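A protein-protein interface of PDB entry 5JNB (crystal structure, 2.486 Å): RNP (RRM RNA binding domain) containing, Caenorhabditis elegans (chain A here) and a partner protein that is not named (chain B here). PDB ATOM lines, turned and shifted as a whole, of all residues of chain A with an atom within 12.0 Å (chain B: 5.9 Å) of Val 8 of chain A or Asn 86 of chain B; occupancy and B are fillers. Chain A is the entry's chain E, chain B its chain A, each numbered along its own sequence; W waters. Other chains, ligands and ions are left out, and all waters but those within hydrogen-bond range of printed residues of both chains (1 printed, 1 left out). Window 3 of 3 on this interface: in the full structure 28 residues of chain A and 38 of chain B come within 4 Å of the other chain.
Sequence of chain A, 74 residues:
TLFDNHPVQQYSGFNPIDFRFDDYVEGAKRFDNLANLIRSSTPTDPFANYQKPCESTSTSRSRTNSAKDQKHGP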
ATOM      1  N   THR A   1      21.681 -26.752  29.094  1.00  0.00           N
ATOM      2  CA  THR A   1      22.158 -25.521  28.471  1.00  0.00           C
ATOM      3  C   THR A   1      21.113 -24.430  28.735  1.00  0.00           C
ATOM      4  O   THR A   1      19.972 -24.711  29.083  1.00  0.00           O
ATOM      5  CB  THR A   1      22.412 -25.714  26.925  1.00  0.00           C
ATOM      6  OG1 THR A   1      23.479 -24.873  26.478  1.00  0.00           O
ATOM      7  CG2 THR A   1      21.159 -25.396  26.082  1.00  0.00           C
ATOM      8  N   LEU A   2      21.547 -23.189  28.627  1.00  0.00           N
ATOM      9  CA  LEU A   2      20.702 -21.993  28.483  1.00  0.00           C
ATOM     10  C   LEU A   2      19.308 -22.154  27.774  1.00  0.00           C
ATOM     11  O   LEU A   2      18.329 -21.471  28.117  1.00  0.00           O
ATOM     12  CB  LEU A   2      21.574 -20.971  27.720  1.00  0.00           C
ATOM     13  CG  LEU A   2      21.025 -19.640  27.223  1.00  0.00           C
ATOM     14  CD1 LEU A   2      20.499 -19.000  28.386  1.00  0.00           C
ATOM     15  CD2 LEU A   2      22.108 -18.764  26.654  1.00  0.00           C
ATOM     16  N   PHE A   3      19.237 -23.044  26.781  1.00  0.00           N
ATOM     17  CA  PHE A   3      18.096 -23.147  25.856  1.00  0.00           C
ATOM     18  C   PHE A   3      16.985 -24.120  26.271  1.00  0.00           C
ATOM     19  O   PHE A   3      15.897 -24.096  25.695  1.00  0.00           O
ATOM     20  CB  PHE A   3      18.608 -23.551  24.454  1.00  0.00           C
ATOM     21  CG  PHE A   3      19.623 -22.596  23.875  1.00  0.00           C
ATOM     22  CD1 PHE A   3      19.362 -21.243  23.804  1.00  0.00           C
ATOM     23  CD2 PHE A   3      20.836 -23.052  23.413  1.00  0.00           C
ATOM     24  CE1 PHE A   3      20.296 -20.363  23.274  1.00  0.00           C
ATOM     25  CE2 PHE A   3      21.769 -22.179  22.893  1.00  0.00           C
ATOM     26  CZ  PHE A   3      21.487 -20.834  22.819  1.00  0.00           C
ATOM     27  N   ASP A   4      17.261 -24.970  27.256  1.00  0.00           N
ATOM     28  CA  ASP A   4      16.293 -25.929  27.806  1.00  0.00           C
ATOM     29  C   ASP A   4      15.647 -26.786  26.742  1.00  0.00           C
ATOM     30  O   ASP A   4      16.192 -26.959  25.675  1.00  0.00           O
ATOM     31  CB  ASP A   4      15.193 -25.216  28.585  1.00  0.00           C
ATOM     32  CG  ASP A   4      15.704 -24.026  29.357  1.00  0.00           C
ATOM     33  OD1 ASP A   4      15.124 -22.922  29.170  1.00  0.00           O
ATOM     34  OD2 ASP A   4      16.679 -24.196  30.144  1.00  0.00           O
ATOM     35  N   ASN A   5      14.462 -27.297  27.024  1.00  0.00           N
ATOM     36  CA  ASN A   5      13.866 -28.286  26.139  1.00  0.00           C
ATOM     37  C   ASN A   5      12.471 -27.913  25.650  1.00  0.00           C
ATOM     38  O   ASN A   5      11.769 -28.758  25.134  1.00  0.00           O
ATOM     39  CB  ASN A   5      13.844 -29.644  26.837  1.00  0.00           C
ATOM     40  CG  ASN A   5      15.211 -30.045  27.304  1.00  0.00           C
ATOM     41  OD1 ASN A   5      16.091 -30.313  26.490  1.00  0.00           O
ATOM     42  ND2 ASN A   5      15.419 -30.055  28.619  1.00  0.00           N
ATOM     43  N   HIS A   6      12.131 -26.631  25.782  1.00  0.00           N
ATOM     44  CA  HIS A   6      10.801 -26.099  25.523  1.00  0.00           C
ATOM     45  C   HIS A   6      10.905 -24.649  25.059  1.00  0.00           C
ATOM     46  O   HIS A   6      11.849 -23.960  25.449  1.00  0.00           O
ATOM     47  CB  HIS A   6       9.942 -26.197  26.785  1.00  0.00           C
ATOM     48  CG  HIS A   6       9.689 -27.603  27.220  1.00  0.00           C
ATOM     49  ND1 HIS A   6      10.577 -28.312  28.000  1.00  0.00           N
ATOM     50  CD2 HIS A   6       8.674 -28.455  26.936  1.00  0.00           C
ATOM     51  CE1 HIS A   6      10.114 -29.530  28.197  1.00  0.00           C
ATOM     52  NE2 HIS A   6       8.958 -29.643  27.561  1.00  0.00           N
ATOM     53  N   PRO A   7       9.936 -24.180  24.235  1.00  0.00           N
ATOM     54  CA  PRO A   7       9.923 -22.777  23.788  1.00  0.00           C
ATOM     55  C   PRO A   7       9.737 -21.826  24.966  1.00  0.00           C
ATOM     56  O   PRO A   7       9.292 -22.263  26.018  1.00  0.00           O
ATOM     57  CB  PRO A   7       8.716 -22.707  22.835  1.00  0.00           C
ATOM     58  CG  PRO A   7       8.350 -24.127  22.519  1.00  0.00           C
ATOM     59  CD  PRO A   7       8.785 -24.941  23.705  1.00  0.00           C
ATOM     60  N   VAL A   8      10.064 -20.550  24.803  1.00  0.00           N
ATOM     61  CA  VAL A   8       9.840 -19.573  25.869  1.00  0.00           C
ATOM     62  C   VAL A   8       8.363 -19.574  26.284  1.00  0.00           C
ATOM     63  O   VAL A   8       7.480 -19.600  25.424  1.00  0.00           O
ATOM     64  CB  VAL A   8      10.257 -18.142  25.430  1.00  0.00           C
ATOM     65  CG1 VAL A   8      10.004 -17.156  26.537  1.00  0.00           C
ATOM     66  CG2 VAL A   8      11.727 -18.107  24.991  1.00  0.00           C
ATOM     67  N   GLN A   9       8.094 -19.562  27.589  1.00  0.00           N
ATOM     68  CA  GLN A   9       6.707 -19.583  28.058  1.00  0.00           C
ATOM     69  C   GLN A   9       6.136 -18.173  28.208  1.00  0.00           C
ATOM     70  O   GLN A   9       4.946 -17.956  27.987  1.00  0.00           O
ATOM     71  CB  GLN A   9       6.586 -20.340  29.381  1.00  0.00           C
ATOM     72  CG  GLN A   9       6.819 -21.848  29.257  1.00  0.00           C
ATOM     73  CD  GLN A   9       5.883 -22.560  28.255  1.00  0.00           C
ATOM     74  OE1 GLN A   9       4.692 -22.762  28.530  1.00  0.00           O
ATOM     75  NE2 GLN A   9       6.441 -22.978  27.104  1.00  0.00           N
ATOM     76  N   GLN A  10       6.984 -17.222  28.588  1.00  0.00           N
ATOM     77  CA  GLN A  10       6.597 -15.817  28.617  1.00  0.00           C
ATOM     78  C   GLN A  10       6.319 -15.354  27.201  1.00  0.00           C
ATOM     79  O   GLN A  10       6.606 -16.076  26.245  1.00  0.00           O
ATOM     80  CB  GLN A  10       7.691 -14.945  29.234  1.00  0.00           C
ATOM     81  CG  GLN A  10       8.102 -15.340  30.634  1.00  0.00           C
ATOM     82  CD  GLN A  10       9.574 -15.055  30.897  1.00  0.00           C
ATOM     83  OE1 GLN A  10      10.274 -14.496  30.046  1.00  0.00           O
ATOM     84  NE2 GLN A  10      10.053 -15.455  32.073  1.00  0.00           N
ATOM     85  N   TYR A  11       5.780 -14.144  27.065  1.00  0.00           N
ATOM     86  CA  TYR A  11       5.582 -13.577  25.743  1.00  0.00           C
ATOM     87  C   TYR A  11       6.914 -13.399  24.990  1.00  0.00           C
ATOM     88  O   TYR A  11       7.748 -12.559  25.342  1.00  0.00           O
ATOM     89  CB  TYR A  11       4.840 -12.236  25.816  1.00  0.00           C
ATOM     90  CG  TYR A  11       4.714 -11.589  24.448  1.00  0.00           C
ATOM     91  CD1 TYR A  11       5.550 -10.536  24.072  1.00  0.00           C
ATOM     92  CD2 TYR A  11       3.783 -12.059  23.516  1.00  0.00           C
ATOM     93  CE1 TYR A  11       5.448  -9.960  22.813  1.00  0.00           C
ATOM     94  CE2 TYR A  11       3.675 -11.490  22.262  1.00  0.00           C
ATOM     95  CZ  TYR A  11       4.508 -10.441  21.915  1.00  0.00           C
ATOM     96  OH  TYR A  11       4.410  -9.876  20.661  1.00  0.00           O
ATOM     97  N   SER A  12       7.104 -14.241  23.978  1.00  0.00           N
ATOM     98  CA  SER A  12       8.061 -14.020  22.899  1.00  0.00           C
ATOM     99  C   SER A  12       7.341 -13.185  21.863  1.00  0.00           C
ATOM    100  O   SER A  12       6.116 -13.239  21.778  1.00  0.00           O
ATOM    101  CB  SER A  12       8.515 -15.341  22.310  1.00  0.00           C
ATOM    102  OG  SER A  12       7.389 -16.200  22.166  1.00  0.00           O
ATOM    103  N   GLY A  13       8.058 -12.426  21.057  1.00  0.00           N
ATOM    104  CA  GLY A  13       7.388 -11.422  20.246  1.00  0.00           C
ATOM    105  C   GLY A  13       6.602 -11.911  19.040  1.00  0.00           C
ATOM    106  O   GLY A  13       6.778 -11.375  17.947  1.00  0.00           O
ATOM    107  N   PHE A  14       5.727 -12.902  19.215  1.00  0.00           N
ATOM    108  CA  PHE A  14       4.943 -13.398  18.077  1.00  0.00           C
ATOM    109  C   PHE A  14       3.991 -12.317  17.590  1.00  0.00           C
ATOM    110  O   PHE A  14       3.490 -11.510  18.375  1.00  0.00           O
ATOM    111  CB  PHE A  14       4.173 -14.685  18.424  1.00  0.00           C
ATOM    112  CG  PHE A  14       3.133 -14.531  19.528  1.00  0.00           C
ATOM    113  CD1 PHE A  14       3.426 -14.911  20.837  1.00  0.00           C
ATOM    114  CD2 PHE A  14       1.853 -14.049  19.245  1.00  0.00           C
ATOM    115  CE1 PHE A  14       2.481 -14.783  21.848  1.00  0.00           C
ATOM    116  CE2 PHE A  14       0.892 -13.919  20.254  1.00  0.00           C
ATOM    117  CZ  PHE A  14       1.210 -14.286  21.561  1.00  0.00           C
ATOM    118  N   ASN A  15       3.763 -12.285  16.284  1.00  0.00           N
ATOM    119  CA  ASN A  15       2.792 -11.348  15.712  1.00  0.00           C
ATOM    120  C   ASN A  15       1.376 -11.754  16.063  1.00  0.00           C
ATOM    121  O   ASN A  15       1.113 -12.930  16.309  1.00  0.00           O
ATOM    122  CB  ASN A  15       2.959 -11.267  14.196  1.00  0.00           C
ATOM    123  CG  ASN A  15       4.295 -10.678  13.797  1.00  0.00           C
ATOM    124  OD1 ASN A  15       5.043 -11.294  13.044  1.00  0.00           O
ATOM    125  ND2 ASN A  15       4.602  -9.474  14.299  1.00  0.00           N
ATOM    126  N   ILE A  17      -2.491 -12.945  16.036  1.00  0.00           N
ATOM    127  CA  ILE A  17      -3.143 -13.984  15.259  1.00  0.00           C
ATOM    128  C   ILE A  17      -4.668 -13.869  15.331  1.00  0.00           C
ATOM    129  O   ILE A  17      -5.256 -14.118  16.373  1.00  0.00           O
ATOM    130  CB  ILE A  17      -2.742 -15.379  15.753  1.00  0.00           C
ATOM    131  CG1 ILE A  17      -1.227 -15.527  15.778  1.00  0.00           C
ATOM    132  CG2 ILE A  17      -3.367 -16.465  14.890  1.00  0.00           C
ATOM    133  CD1 ILE A  17      -0.795 -16.882  16.221  1.00  0.00           C
ATOM    134  N   PHE A  19      -8.152 -15.141  15.097  1.00  0.00           N
ATOM    135  CA  PHE A  19      -8.953 -16.359  15.028  1.00  0.00           C
ATOM    136  C   PHE A  19     -10.449 -16.081  14.841  1.00  0.00           C
ATOM    137  O   PHE A  19     -11.112 -15.481  15.699  1.00  0.00           O
ATOM    138  CB  PHE A  19      -8.766 -17.207  16.283  1.00  0.00           C
ATOM    139  CG  PHE A  19      -7.495 -17.971  16.305  1.00  0.00           C
ATOM    140  CD1 PHE A  19      -7.343 -19.099  15.525  1.00  0.00           C
ATOM    141  CD2 PHE A  19      -6.444 -17.570  17.112  1.00  0.00           C
ATOM    142  CE1 PHE A  19      -6.163 -19.820  15.551  1.00  0.00           C
ATOM    143  CE2 PHE A  19      -5.258 -18.280  17.134  1.00  0.00           C
ATOM    144  CZ  PHE A  19      -5.117 -19.408  16.351  1.00  0.00           C
ATOM    145  N   ALA B  81       1.213 -21.850  13.941  1.00  0.00           N
ATOM    146  CA  ALA B  81       0.881 -23.129  14.576  1.00  0.00           C
ATOM    147  C   ALA B  81       1.759 -23.361  15.810  1.00  0.00           C
ATOM    148  O   ALA B  81       1.376 -24.079  16.741  1.00  0.00           O
ATOM    149  CB  ALA B  81       1.019 -24.277  13.595  1.00  0.00           C
ATOM    150  N   VAL B  82       2.923 -22.734  15.825  1.00  0.00           N
ATOM    151  CA  VAL B  82       3.822 -22.861  16.960  1.00  0.00           C
ATOM    152  C   VAL B  82       3.265 -22.119  18.174  1.00  0.00           C
ATOM    153  O   VAL B  82       3.247 -22.662  19.280  1.00  0.00           O
ATOM    154  CB  VAL B  82       5.232 -22.351  16.589  1.00  0.00           C
ATOM    155  CG1 VAL B  82       6.172 -22.513  17.723  1.00  0.00           C
ATOM    156  CG2 VAL B  82       5.735 -23.117  15.378  1.00  0.00           C
ATOM    157  N   VAL B  83       2.781 -20.895  17.962  1.00  0.00           N
ATOM    158  CA  VAL B  83       2.054 -20.173  19.008  1.00  0.00           C
ATOM    159  C   VAL B  83       0.888 -21.005  19.599  1.00  0.00           C
ATOM    160  O   VAL B  83       0.814 -21.189  20.809  1.00  0.00           O
ATOM    161  CB  VAL B  83       1.517 -18.812  18.471  1.00  0.00           C
ATOM    162  CG1 VAL B  83       0.737 -18.066  19.551  1.00  0.00           C
ATOM    163  CG2 VAL B  83       2.677 -17.948  17.963  1.00  0.00           C
ATOM    164  N   VAL B  84      -0.008 -21.517  18.754  1.00  0.00           N
ATOM    165  CA  VAL B  84      -1.108 -22.369  19.216  1.00  0.00           C
ATOM    166  C   VAL B  84      -0.661 -23.620  19.980  1.00  0.00           C
ATOM    167  O   VAL B  84      -1.178 -23.908  21.042  1.00  0.00           O
ATOM    168  CB  VAL B  84      -1.989 -22.818  18.046  1.00  0.00           C
ATOM    169  CG1 VAL B  84      -3.125 -23.701  18.550  1.00  0.00           C
ATOM    170  CG2 VAL B  84      -2.544 -21.621  17.342  1.00  0.00           C
ATOM    171  N   LEU B  85       0.290 -24.372  19.445  1.00  0.00           N
ATOM    172  CA  LEU B  85       0.812 -25.546  20.168  1.00  0.00           C
ATOM    173  C   LEU B  85       1.495 -25.174  21.483  1.00  0.00           C
ATOM    174  O   LEU B  85       1.433 -25.931  22.461  1.00  0.00           O
ATOM    175  CB  LEU B  85       1.787 -26.335  19.296  1.00  0.00           C
ATOM    176  CG  LEU B  85       1.062 -26.939  18.085  1.00  0.00           C
ATOM    177  CD1 LEU B  85       1.983 -27.674  17.100  1.00  0.00           C
ATOM    178  CD2 LEU B  85      -0.093 -27.825  18.579  1.00  0.00           C
ATOM    179  N   ASN B  86       2.143 -24.013  21.514  1.00  0.00           N
ATOM    180  CA  ASN B  86       2.841 -23.593  22.728  1.00  0.00           C
ATOM    181  C   ASN B  86       1.833 -23.125  23.748  1.00  0.00           C
ATOM    182  O   ASN B  86       2.032 -23.309  24.956  1.00  0.00           O
ATOM    183  CB  ASN B  86       3.874 -22.486  22.451  1.00  0.00           C
ATOM    184  CG  ASN B  86       4.793 -22.237  23.650  1.00  0.00           C
ATOM    185  OD1 ASN B  86       5.348 -23.177  24.240  1.00  0.00           O
ATOM    186  ND2 ASN B  86       4.943 -20.975  24.025  1.00  0.00           N
ATOM    187  N   LEU B  87       0.736 -22.536  23.262  1.00  0.00           N
ATOM    188  CA  LEU B  87      -0.323 -22.103  24.152  1.00  0.00           C
ATOM    189  C   LEU B  87      -0.981 -23.323  24.781  1.00  0.00           C
ATOM    190  O   LEU B  87      -1.303 -23.315  25.956  1.00  0.00           O
ATOM    191  CB  LEU B  87      -1.332 -21.240  23.413  1.00  0.00           C
ATOM    192  CG  LEU B  87      -2.536 -20.785  24.245  1.00  0.00           C
ATOM    193  CD1 LEU B  87      -2.073 -20.124  25.549  1.00  0.00           C
ATOM    194  CD2 LEU B  87      -3.446 -19.855  23.415  1.00  0.00           C
ATOM    195  N   ILE B  88      -1.119 -24.390  24.005  1.00  0.00           N
ATOM    196  CA  ILE B  88      -1.770 -25.612  24.467  1.00  0.00           C
ATOM    197  C   ILE B  88      -0.873 -26.369  25.421  1.00  0.00           C
ATOM    198  O   ILE B  88      -1.341 -26.979  26.380  1.00  0.00           O
ATOM    199  CB  ILE B  88      -2.146 -26.523  23.273  1.00  0.00           C
ATOM    200  CG1 ILE B  88      -3.287 -25.913  22.479  1.00  0.00           C
ATOM    201  CG2 ILE B  88      -2.546 -27.922  23.734  1.00  0.00           C
ATOM    202  CD1 ILE B  88      -3.533 -26.642  21.180  1.00  0.00           C
ATOM    203  N   LEU B  89       0.425 -26.334  25.140  1.00  0.00           N
ATOM    204  CA  LEU B  89       1.438 -26.867  26.042  1.00  0.00           C
ATOM    205  C   LEU B  89       1.315 -26.220  27.423  1.00  0.00           C
ATOM    206  O   LEU B  89       1.268 -26.930  28.426  1.00  0.00           O
ATOM    207  CB  LEU B  89       2.833 -26.637  25.458  1.00  0.00           C
ATOM    208  CG  LEU B  89       4.096 -27.210  26.116  1.00  0.00           C
ATOM    209  CD1 LEU B  89       5.163 -27.332  25.061  1.00  0.00           C
ATOM    210  CD2 LEU B  89       4.597 -26.340  27.264  1.00  0.00           C
ATOM    211  N   SER B  90       1.272 -24.882  27.463  1.00  0.00           N
ATOM    212  CA  SER B  90       1.072 -24.117  28.708  1.00  0.00           C
ATOM    213  C   SER B  90      -0.135 -24.617  29.483  1.00  0.00           C
ATOM    214  O   SER B  90      -0.069 -24.806  30.684  1.00  0.00           O
ATOM    215  CB  SER B  90       0.862 -22.620  28.429  1.00  0.00           C
ATOM    216  OG  SER B  90       2.023 -21.982  27.921  1.00  0.00           O
ATOM    217  N   THR B  91      -1.245 -24.819  28.774  1.00  0.00           N
ATOM    218  CA  THR B  91      -2.503 -25.199  29.404  1.00  0.00           C
ATOM    219  C   THR B  91      -2.462 -26.646  29.913  1.00  0.00           C
ATOM    220  O   THR B  91      -2.951 -26.939  30.994  1.00  0.00           O
ATOM    221  CB  THR B  91      -3.688 -24.987  28.419  1.00  0.00           C
ATOM    222  OG1 THR B  91      -3.918 -23.578  28.254  1.00  0.00           O
ATOM    223  CG2 THR B  91      -4.972 -25.654  28.929  1.00  0.00           C
ATOM    224  N   LEU B 103       7.733 -29.963  21.770  1.00  0.00           N
ATOM    225  CA  LEU B 103       7.402 -29.520  20.424  1.00  0.00           C
ATOM    226  C   LEU B 103       8.421 -30.026  19.394  1.00  0.00           C
ATOM    227  O   LEU B 103       9.591 -29.656  19.418  1.00  0.00           O
ATOM    228  CB  LEU B 103       7.293 -27.987  20.378  1.00  0.00           C
ATOM    229  CG  LEU B 103       5.849 -27.499  20.222  1.00  0.00           C
ATOM    230  CD1 LEU B 103       5.691 -25.991  20.324  1.00  0.00           C
ATOM    231  CD2 LEU B 103       5.319 -27.973  18.883  1.00  0.00           C
HETATM  232  O   HOH W   1       9.891 -28.509  22.941  1.00  0.00           O
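Printed residues of chain B that touch a printed residue of chain A: Val 83, Val 84, Asn 86, Leu 89, Ser 90 and Leu 103. Hydrophobic or aromatic side chains of chain B within 4 Å of the printed part of chain A: Val 83, Val 84, Leu 89 and Leu 103. Of the 17 printed residues of chain A, 6 touch a printed residue of chain B. Printed residues of chain A that touch a printed residue of chain B: Pro 7, Val 8, Gln 9, Phe 14, Ile 17 and Phe 19. Hydrophobic or aromatic side chains of chain A that line the printed part of chain B: Pro 7, Phe 14, Ile 17 and Phe 19. Along chain A the printed residues that touch a printed residue of chain B span positions 7 to 19. Among the printed residues, 9 pairs touch across the chains.
Val 8 of chain A touches one residue of chain B. Gln 10 of chain A touches none of the printed residues of chain B. Printed residues of chain B within 4 Å of Phe 14 of chain A: Val 83 (3.6 Å). Asn 15 of chain A touches none of the printed residues of chain B. Val 84 of chain B touches one residue of chain A. No residue of chain A comes within 4 Å of Ile 88 of chain B. Of the printed residues of chain A, Leu 103 of chain B touches Pro 7. The nearest printed residue of chain B that does not touch Val 8 of chain A is Ser 90 of chain B (6.5 Å). The nearest printed residue of chain A that does not touch Leu 103 of chain B is Asn 5 of chain A (5.4 Å).
The backbone carbonyl oxygen (O) of Asn 86 of chain B sits at hydrogen-bond distance from the side-chain hydroxyl (OG) of Ser 90 of chain B, 3.2 Å away. The side-chain amide nitrogen (NE2) of Gln 9 of chain A is in hydrogen-bond range of the backbone carbonyl oxygen (O) of Pro 7 of chain A (3.1 Å). The side-chain hydroxyl (OH) of Tyr 11 of chain A is in hydrogen-bond range of the backbone carbonyl oxygen (O) of Phe 14 of chain A (3.0 Å).
Among the printed residues, merely in contact across the chains: Phe 19 of chain A with Val 84 of chain B (3.5 Å), Pro 7 of chain A with Asn 86 of chain B (3.6 Å), Phe 14 of chain A with Val 83 of chain B (3.6 Å), Ile 17 of chain A with Val 83 of chain B (3.8 Å), Gln 9 of chain A with Leu 89 of chain B (3.8 Å) and Pro 7 of chain A with Leu 103 of chain B (3.9 Å).
Water W1 lies within hydrogen-bond range of the backbone NH of Leu 103 of chain B (2.9 Å) and the backbone carbonyl oxygen of Asn 5 of chain A (2.9 Å).
O of Val 8 of chain A sits at hydrogen-bond distance from ND2 of Asn 86 of chain B. OD1 of Asn 86 of chain B lies within hydrogen-bond range of NE2 of Gln 9 of chain A, at 3.1 Å. OE1 of Gln 9 of chain A is in hydrogen-bond range of OG of Ser 90 of chain B (2.8 Å).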
